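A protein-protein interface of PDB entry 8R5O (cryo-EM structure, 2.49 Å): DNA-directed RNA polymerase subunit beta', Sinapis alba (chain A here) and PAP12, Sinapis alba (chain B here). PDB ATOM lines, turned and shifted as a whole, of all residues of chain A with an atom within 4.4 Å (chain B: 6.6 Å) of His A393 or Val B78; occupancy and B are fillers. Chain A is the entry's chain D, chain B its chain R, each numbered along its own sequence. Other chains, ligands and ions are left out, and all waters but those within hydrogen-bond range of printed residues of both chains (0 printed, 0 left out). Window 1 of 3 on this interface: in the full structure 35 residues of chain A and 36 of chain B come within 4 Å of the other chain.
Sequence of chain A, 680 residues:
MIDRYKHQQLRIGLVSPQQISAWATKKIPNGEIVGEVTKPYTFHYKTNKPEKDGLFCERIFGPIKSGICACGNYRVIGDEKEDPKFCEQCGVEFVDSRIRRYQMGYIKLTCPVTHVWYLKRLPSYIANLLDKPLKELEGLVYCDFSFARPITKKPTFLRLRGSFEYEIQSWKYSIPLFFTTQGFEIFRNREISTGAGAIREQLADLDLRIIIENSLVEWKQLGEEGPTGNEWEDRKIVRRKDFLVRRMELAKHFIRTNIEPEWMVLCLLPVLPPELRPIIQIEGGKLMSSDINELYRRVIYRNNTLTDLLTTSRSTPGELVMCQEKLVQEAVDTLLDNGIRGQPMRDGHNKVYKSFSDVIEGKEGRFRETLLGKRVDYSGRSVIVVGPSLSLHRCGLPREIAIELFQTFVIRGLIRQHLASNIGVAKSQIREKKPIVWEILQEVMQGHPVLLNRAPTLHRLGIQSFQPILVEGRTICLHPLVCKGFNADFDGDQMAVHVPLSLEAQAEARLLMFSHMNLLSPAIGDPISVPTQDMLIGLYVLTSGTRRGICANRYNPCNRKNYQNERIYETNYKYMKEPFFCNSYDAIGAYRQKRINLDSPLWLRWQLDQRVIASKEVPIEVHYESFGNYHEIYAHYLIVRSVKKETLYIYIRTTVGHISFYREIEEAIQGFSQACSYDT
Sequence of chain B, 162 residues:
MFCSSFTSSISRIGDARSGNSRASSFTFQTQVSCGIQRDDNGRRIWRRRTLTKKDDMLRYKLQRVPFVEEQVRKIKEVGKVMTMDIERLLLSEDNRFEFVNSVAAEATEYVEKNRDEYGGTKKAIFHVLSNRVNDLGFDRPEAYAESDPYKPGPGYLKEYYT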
ATOM      1  N   SER A 391      26.273 -21.814  12.241  1.00  0.00           N
ATOM      2  CA  SER A 391      27.355 -20.940  12.660  1.00  0.00           C
ATOM      3  C   SER A 391      28.609 -21.766  12.941  1.00  0.00           C
ATOM      4  O   SER A 391      28.572 -22.994  13.044  1.00  0.00           O
ATOM      5  CB  SER A 391      26.951 -20.138  13.895  1.00  0.00           C
ATOM      6  OG  SER A 391      25.750 -19.423  13.669  1.00  0.00           O
ATOM      7  N   LEU A 392      29.739 -21.069  13.062  1.00  0.00           N
ATOM      8  CA  LEU A 392      31.001 -21.750  13.328  1.00  0.00           C
ATOM      9  C   LEU A 392      31.009 -22.424  14.695  1.00  0.00           C
ATOM     10  O   LEU A 392      31.690 -23.438  14.881  1.00  0.00           O
ATOM     11  CB  LEU A 392      32.159 -20.761  13.219  1.00  0.00           C
ATOM     12  CG  LEU A 392      32.739 -20.552  11.821  1.00  0.00           C
ATOM     13  CD1 LEU A 392      33.553 -19.270  11.758  1.00  0.00           C
ATOM     14  CD2 LEU A 392      33.598 -21.745  11.449  1.00  0.00           C
ATOM     15  N   HIS A 393      30.263 -21.886  15.656  1.00  0.00           N
ATOM     16  CA  HIS A 393      30.290 -22.362  17.030  1.00  0.00           C
ATOM     17  C   HIS A 393      29.124 -23.280  17.370  1.00  0.00           C
ATOM     18  O   HIS A 393      28.965 -23.650  18.536  1.00  0.00           O
ATOM     19  CB  HIS A 393      30.304 -21.172  17.988  1.00  0.00           C
ATOM     20  CG  HIS A 393      29.030 -20.389  17.992  1.00  0.00           C
ATOM     21  ND1 HIS A 393      28.613 -19.640  16.913  1.00  0.00           N
ATOM     22  CD2 HIS A 393      28.077 -20.243  18.943  1.00  0.00           C
ATOM     23  CE1 HIS A 393      27.459 -19.064  17.199  1.00  0.00           C
ATOM     24  NE2 HIS A 393      27.113 -19.413  18.425  1.00  0.00           N
ATOM     25  N   ARG A 394      28.307 -23.656  16.393  1.00  0.00           N
ATOM     26  CA  ARG A 394      27.105 -24.429  16.658  1.00  0.00           C
ATOM     27  C   ARG A 394      27.142 -25.760  15.920  1.00  0.00           C
ATOM     28  O   ARG A 394      27.878 -25.942  14.948  1.00  0.00           O
ATOM     29  CB  ARG A 394      25.847 -23.644  16.268  1.00  0.00           C
ATOM     30  CG  ARG A 394      25.783 -22.266  16.898  1.00  0.00           C
ATOM     31  CD  ARG A 394      24.433 -21.987  17.532  1.00  0.00           C
ATOM     32  NE  ARG A 394      23.389 -21.781  16.536  1.00  0.00           N
ATOM     33  CZ  ARG A 394      22.160 -21.371  16.817  1.00  0.00           C
ATOM     34  NH1 ARG A 394      21.790 -21.103  18.058  1.00  0.00           N
ATOM     35  NH2 ARG A 394      21.285 -21.220  15.828  1.00  0.00           N
ATOM     36  N   PHE A 466      31.115 -27.249  20.755  1.00  0.00           N
ATOM     37  CA  PHE A 466      30.080 -26.550  20.011  1.00  0.00           C
ATOM     38  C   PHE A 466      28.861 -26.369  20.899  1.00  0.00           C
ATOM     39  O   PHE A 466      28.657 -27.104  21.866  1.00  0.00           O
ATOM     40  CB  PHE A 466      29.670 -27.309  18.737  1.00  0.00           C
ATOM     41  CG  PHE A 466      30.813 -27.628  17.820  1.00  0.00           C
ATOM     42  CD1 PHE A 466      31.541 -28.792  17.987  1.00  0.00           C
ATOM     43  CD2 PHE A 466      31.153 -26.773  16.789  1.00  0.00           C
ATOM     44  CE1 PHE A 466      32.594 -29.093  17.146  1.00  0.00           C
ATOM     45  CE2 PHE A 466      32.205 -27.068  15.945  1.00  0.00           C
ATOM     46  CZ  PHE A 466      32.925 -28.229  16.125  1.00  0.00           C
ATOM     47  N   GLN A 467      28.050 -25.371  20.563  1.00  0.00           N
ATOM     48  CA  GLN A 467      26.754 -25.209  21.200  1.00  0.00           C
ATOM     49  C   GLN A 467      25.721 -26.015  20.425  1.00  0.00           C
ATOM     50  O   GLN A 467      25.437 -25.680  19.270  1.00  0.00           O
ATOM     51  CB  GLN A 467      26.353 -23.744  21.245  1.00  0.00           C
ATOM     52  CG  GLN A 467      24.934 -23.505  21.720  1.00  0.00           C
ATOM     53  CD  GLN A 467      24.674 -24.079  23.096  1.00  0.00           C
ATOM     54  OE1 GLN A 467      23.745 -24.862  23.287  1.00  0.00           O
ATOM     55  NE2 GLN A 467      25.489 -23.687  24.067  1.00  0.00           N
ATOM     56  N   PHE A 514      36.051 -23.417  22.337  1.00  0.00           N
ATOM     57  CA  PHE A 514      35.099 -23.029  21.307  1.00  0.00           C
ATOM     58  C   PHE A 514      35.823 -22.638  20.020  1.00  0.00           C
ATOM     59  O   PHE A 514      36.997 -22.262  20.021  1.00  0.00           O
ATOM     60  CB  PHE A 514      34.209 -21.887  21.794  1.00  0.00           C
ATOM     61  CG  PHE A 514      32.774 -22.277  21.971  1.00  0.00           C
ATOM     62  CD1 PHE A 514      32.426 -23.336  22.789  1.00  0.00           C
ATOM     63  CD2 PHE A 514      31.770 -21.582  21.322  1.00  0.00           C
ATOM     64  CE1 PHE A 514      31.104 -23.698  22.954  1.00  0.00           C
ATOM     65  CE2 PHE A 514      30.449 -21.937  21.483  1.00  0.00           C
ATOM     66  CZ  PHE A 514      30.115 -22.996  22.300  1.00  0.00           C
ATOM     67  N   HIS A 516      35.988 -20.258  17.989  1.00  0.00           N
ATOM     68  CA  HIS A 516      36.269 -18.883  17.599  1.00  0.00           C
ATOM     69  C   HIS A 516      37.440 -18.254  18.336  1.00  0.00           C
ATOM     70  O   HIS A 516      37.941 -17.223  17.878  1.00  0.00           O
ATOM     71  CB  HIS A 516      35.026 -17.999  17.793  1.00  0.00           C
ATOM     72  CG  HIS A 516      34.442 -18.069  19.169  1.00  0.00           C
ATOM     73  ND1 HIS A 516      35.022 -17.457  20.259  1.00  0.00           N
ATOM     74  CD2 HIS A 516      33.325 -18.679  19.632  1.00  0.00           C
ATOM     75  CE1 HIS A 516      34.290 -17.687  21.333  1.00  0.00           C
ATOM     76  NE2 HIS A 516      33.253 -18.426  20.979  1.00  0.00           N
ATOM     77  N   ARG B  73      20.130  -9.070  13.923  1.00  0.00           N
ATOM     78  CA  ARG B  73      19.204  -9.937  14.640  1.00  0.00           C
ATOM     79  C   ARG B  73      19.677 -11.385  14.644  1.00  0.00           C
ATOM     80  O   ARG B  73      19.441 -12.107  15.618  1.00  0.00           O
ATOM     81  CB  ARG B  73      17.801  -9.809  14.041  1.00  0.00           C
ATOM     82  CG  ARG B  73      17.134 -11.117  13.653  1.00  0.00           C
ATOM     83  CD  ARG B  73      15.648 -10.922  13.399  1.00  0.00           C
ATOM     84  NE  ARG B  73      15.367  -9.688  12.676  1.00  0.00           N
ATOM     85  CZ  ARG B  73      15.357  -9.576  11.355  1.00  0.00           C
ATOM     86  NH1 ARG B  73      15.622 -10.607  10.572  1.00  0.00           N
ATOM     87  NH2 ARG B  73      15.073  -8.399  10.807  1.00  0.00           N
ATOM     88  N   LYS B  74      20.362 -11.823  13.585  1.00  0.00           N
ATOM     89  CA  LYS B  74      20.889 -13.184  13.568  1.00  0.00           C
ATOM     90  C   LYS B  74      22.087 -13.330  14.498  1.00  0.00           C
ATOM     91  O   LYS B  74      22.294 -14.398  15.086  1.00  0.00           O
ATOM     92  CB  LYS B  74      21.266 -13.593  12.145  1.00  0.00           C
ATOM     93  CG  LYS B  74      20.089 -14.031  11.295  1.00  0.00           C
ATOM     94  CD  LYS B  74      20.551 -14.808  10.074  1.00  0.00           C
ATOM     95  CE  LYS B  74      19.378 -15.456   9.357  1.00  0.00           C
ATOM     96  NZ  LYS B  74      19.822 -16.330   8.239  1.00  0.00           N
ATOM     97  N   ILE B  75      22.895 -12.277  14.631  1.00  0.00           N
ATOM     98  CA  ILE B  75      24.040 -12.325  15.537  1.00  0.00           C
ATOM     99  C   ILE B  75      23.574 -12.563  16.968  1.00  0.00           C
ATOM    100  O   ILE B  75      24.158 -13.369  17.702  1.00  0.00           O
ATOM    101  CB  ILE B  75      24.871 -11.034  15.412  1.00  0.00           C
ATOM    102  CG1 ILE B  75      25.625 -11.011  14.082  1.00  0.00           C
ATOM    103  CG2 ILE B  75      25.842 -10.898  16.572  1.00  0.00           C
ATOM    104  CD1 ILE B  75      26.382  -9.732  13.834  1.00  0.00           C
ATOM    105  N   LYS B  76      22.509 -11.875  17.383  1.00  0.00           N
ATOM    106  CA  LYS B  76      21.964 -12.090  18.719  1.00  0.00           C
ATOM    107  C   LYS B  76      21.347 -13.478  18.854  1.00  0.00           C
ATOM    108  O   LYS B  76      21.439 -14.101  19.918  1.00  0.00           O
ATOM    109  CB  LYS B  76      20.930 -11.013  19.042  1.00  0.00           C
ATOM    110  CG  LYS B  76      21.455  -9.595  18.940  1.00  0.00           C
ATOM    111  CD  LYS B  76      20.340  -8.587  19.154  1.00  0.00           C
ATOM    112  CE  LYS B  76      20.845  -7.160  19.032  1.00  0.00           C
ATOM    113  NZ  LYS B  76      21.826  -6.824  20.096  1.00  0.00           N
ATOM    114  N   GLU B  77      20.703 -13.973  17.794  1.00  0.00           N
ATOM    115  CA  GLU B  77      20.048 -15.277  17.862  1.00  0.00           C
ATOM    116  C   GLU B  77      21.054 -16.402  18.069  1.00  0.00           C
ATOM    117  O   GLU B  77      20.793 -17.346  18.823  1.00  0.00           O
ATOM    118  CB  GLU B  77      19.228 -15.525  16.597  1.00  0.00           C
ATOM    119  CG  GLU B  77      17.938 -14.724  16.521  1.00  0.00           C
ATOM    120  CD  GLU B  77      17.218 -14.902  15.196  1.00  0.00           C
ATOM    121  OE1 GLU B  77      17.632 -15.773  14.403  1.00  0.00           O
ATOM    122  OE2 GLU B  77      16.240 -14.167  14.947  1.00  0.00           O
ATOM    123  N   VAL B  78      22.211 -16.325  17.404  1.00  0.00           N
ATOM    124  CA  VAL B  78      23.192 -17.403  17.480  1.00  0.00           C
ATOM    125  C   VAL B  78      24.118 -17.282  18.681  1.00  0.00           C
ATOM    126  O   VAL B  78      24.907 -18.205  18.936  1.00  0.00           O
ATOM    127  CB  VAL B  78      24.037 -17.475  16.193  1.00  0.00           C
ATOM    128  CG1 VAL B  78      23.145 -17.713  14.989  1.00  0.00           C
ATOM    129  CG2 VAL B  78      24.843 -16.206  16.018  1.00  0.00           C
ATOM    130  N   GLY B  79      24.051 -16.185  19.429  1.00  0.00           N
ATOM    131  CA  GLY B  79      24.879 -16.027  20.605  1.00  0.00           C
ATOM    132  C   GLY B  79      26.254 -15.458  20.360  1.00  0.00           C
ATOM    133  O   GLY B  79      27.147 -15.655  21.192  1.00  0.00           O
ATOM    134  N   LYS B  80      26.462 -14.762  19.242  1.00  0.00           N
ATOM    135  CA  LYS B  80      27.767 -14.179  18.959  1.00  0.00           C
ATOM    136  C   LYS B  80      28.076 -12.981  19.843  1.00  0.00           C
ATOM    137  O   LYS B  80      29.243 -12.587  19.938  1.00  0.00           O
ATOM    138  CB  LYS B  80      27.852 -13.771  17.489  1.00  0.00           C
ATOM    139  CG  LYS B  80      28.098 -14.923  16.539  1.00  0.00           C
ATOM    140  CD  LYS B  80      28.067 -14.457  15.093  1.00  0.00           C
ATOM    141  CE  LYS B  80      28.378 -15.598  14.145  1.00  0.00           C
ATOM    142  NZ  LYS B  80      28.157 -15.229  12.723  1.00  0.00           N
ATOM    143  N   VAL B  81      27.065 -12.386  20.478  1.00  0.00           N
ATOM    144  CA  VAL B  81      27.303 -11.228  21.334  1.00  0.00           C
ATOM    145  C   VAL B  81      28.171 -11.617  22.524  1.00  0.00           C
ATOM    146  O   VAL B  81      29.127 -10.917  22.873  1.00  0.00           O
ATOM    147  CB  VAL B  81      25.969 -10.607  21.786  1.00  0.00           C
ATOM    148  CG1 VAL B  81      26.218  -9.484  22.778  1.00  0.00           C
ATOM    149  CG2 VAL B  81      25.193 -10.101  20.586  1.00  0.00           C
ATOM    150  N   THR B  83      30.246 -13.999  22.612  1.00  0.00           N
ATOM    151  CA  THR B  83      31.584 -14.279  22.102  1.00  0.00           C
ATOM    152  C   THR B  83      32.459 -13.033  22.141  1.00  0.00           C
ATOM    153  O   THR B  83      33.624 -13.094  22.546  1.00  0.00           O
ATOM    154  CB  THR B  83      31.494 -14.829  20.677  1.00  0.00           C
ATOM    155  OG1 THR B  83      30.963 -16.159  20.705  1.00  0.00           O
ATOM    156  CG2 THR B  83      32.858 -14.841  20.009  1.00  0.00           C
ATOM    157  N   TYR B 160      14.631 -26.379  13.164  1.00  0.00           N
ATOM    158  CA  TYR B 160      15.801 -25.881  12.457  1.00  0.00           C
ATOM    159  C   TYR B 160      15.994 -26.605  11.130  1.00  0.00           C
ATOM    160  O   TYR B 160      16.077 -27.832  11.090  1.00  0.00           O
ATOM    161  CB  TYR B 160      17.049 -26.029  13.327  1.00  0.00           C
ATOM    162  CG  TYR B 160      18.228 -25.226  12.836  1.00  0.00           C
ATOM    163  CD1 TYR B 160      18.385 -23.898  13.204  1.00  0.00           C
ATOM    164  CD2 TYR B 160      19.184 -25.793  12.005  1.00  0.00           C
ATOM    165  CE1 TYR B 160      19.458 -23.157  12.759  1.00  0.00           C
ATOM    166  CE2 TYR B 160      20.263 -25.059  11.556  1.00  0.00           C
ATOM    167  CZ  TYR B 160      20.394 -23.741  11.937  1.00  0.00           C
ATOM    168  OH  TYR B 160      21.463 -23.000  11.496  1.00  0.00           O
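The backbone carbonyl oxygen (O) of Val B78 lies within hydrogen-bond range of a ring nitrogen (NE2) of His A393. The side-chain hydroxyl of Thr B83 sits at hydrogen-bond distance from a ring nitrogen (NE2) of His A516 (3.2 Å).
Val B78 touches Ser A391. Arg A394 touches Glu B77. NH1 of Arg A394 touches CA of Val B78 (3.999 Å).
Of chain B, only Val B78 comes within 4 Å of His A393. Of the printed residues of chain A, Val B78 touches Ser A391 (3.4 Å), His A393 (2.6 Å) and Arg A394 (3.999 Å). Printed residues of chain B within 4 Å of Arg A394: Glu B77 and Val B78. Of the printed residues of chain B, His A516 touches Thr B83. Printed residues of chain A within 4 Å of Glu B77: Arg A394. Printed residues of chain A within 4 Å of Thr B83: His A516 (3.2 Å). Printed residues of chain B within 4 Å of Ser A391: Val B78 (3.4 Å). The nearest printed residue of chain A that does not touch Val B78 is Gln A467 (6.0 Å).
The backbone carbonyl oxygen of His A393 sits at hydrogen-bond distance from the backbone NH of Gln A467.
Of the 8 printed residues of chain A, 4 touch a printed residue of chain B. Of the 11 printed residues of chain B, 3 touch a printed residue of chain A. Hydrophobic or aromatic side chains of chain B within 4 Å of the printed part of chain A: Val B78. Among the printed residues, 5 pairs touch across the chains.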
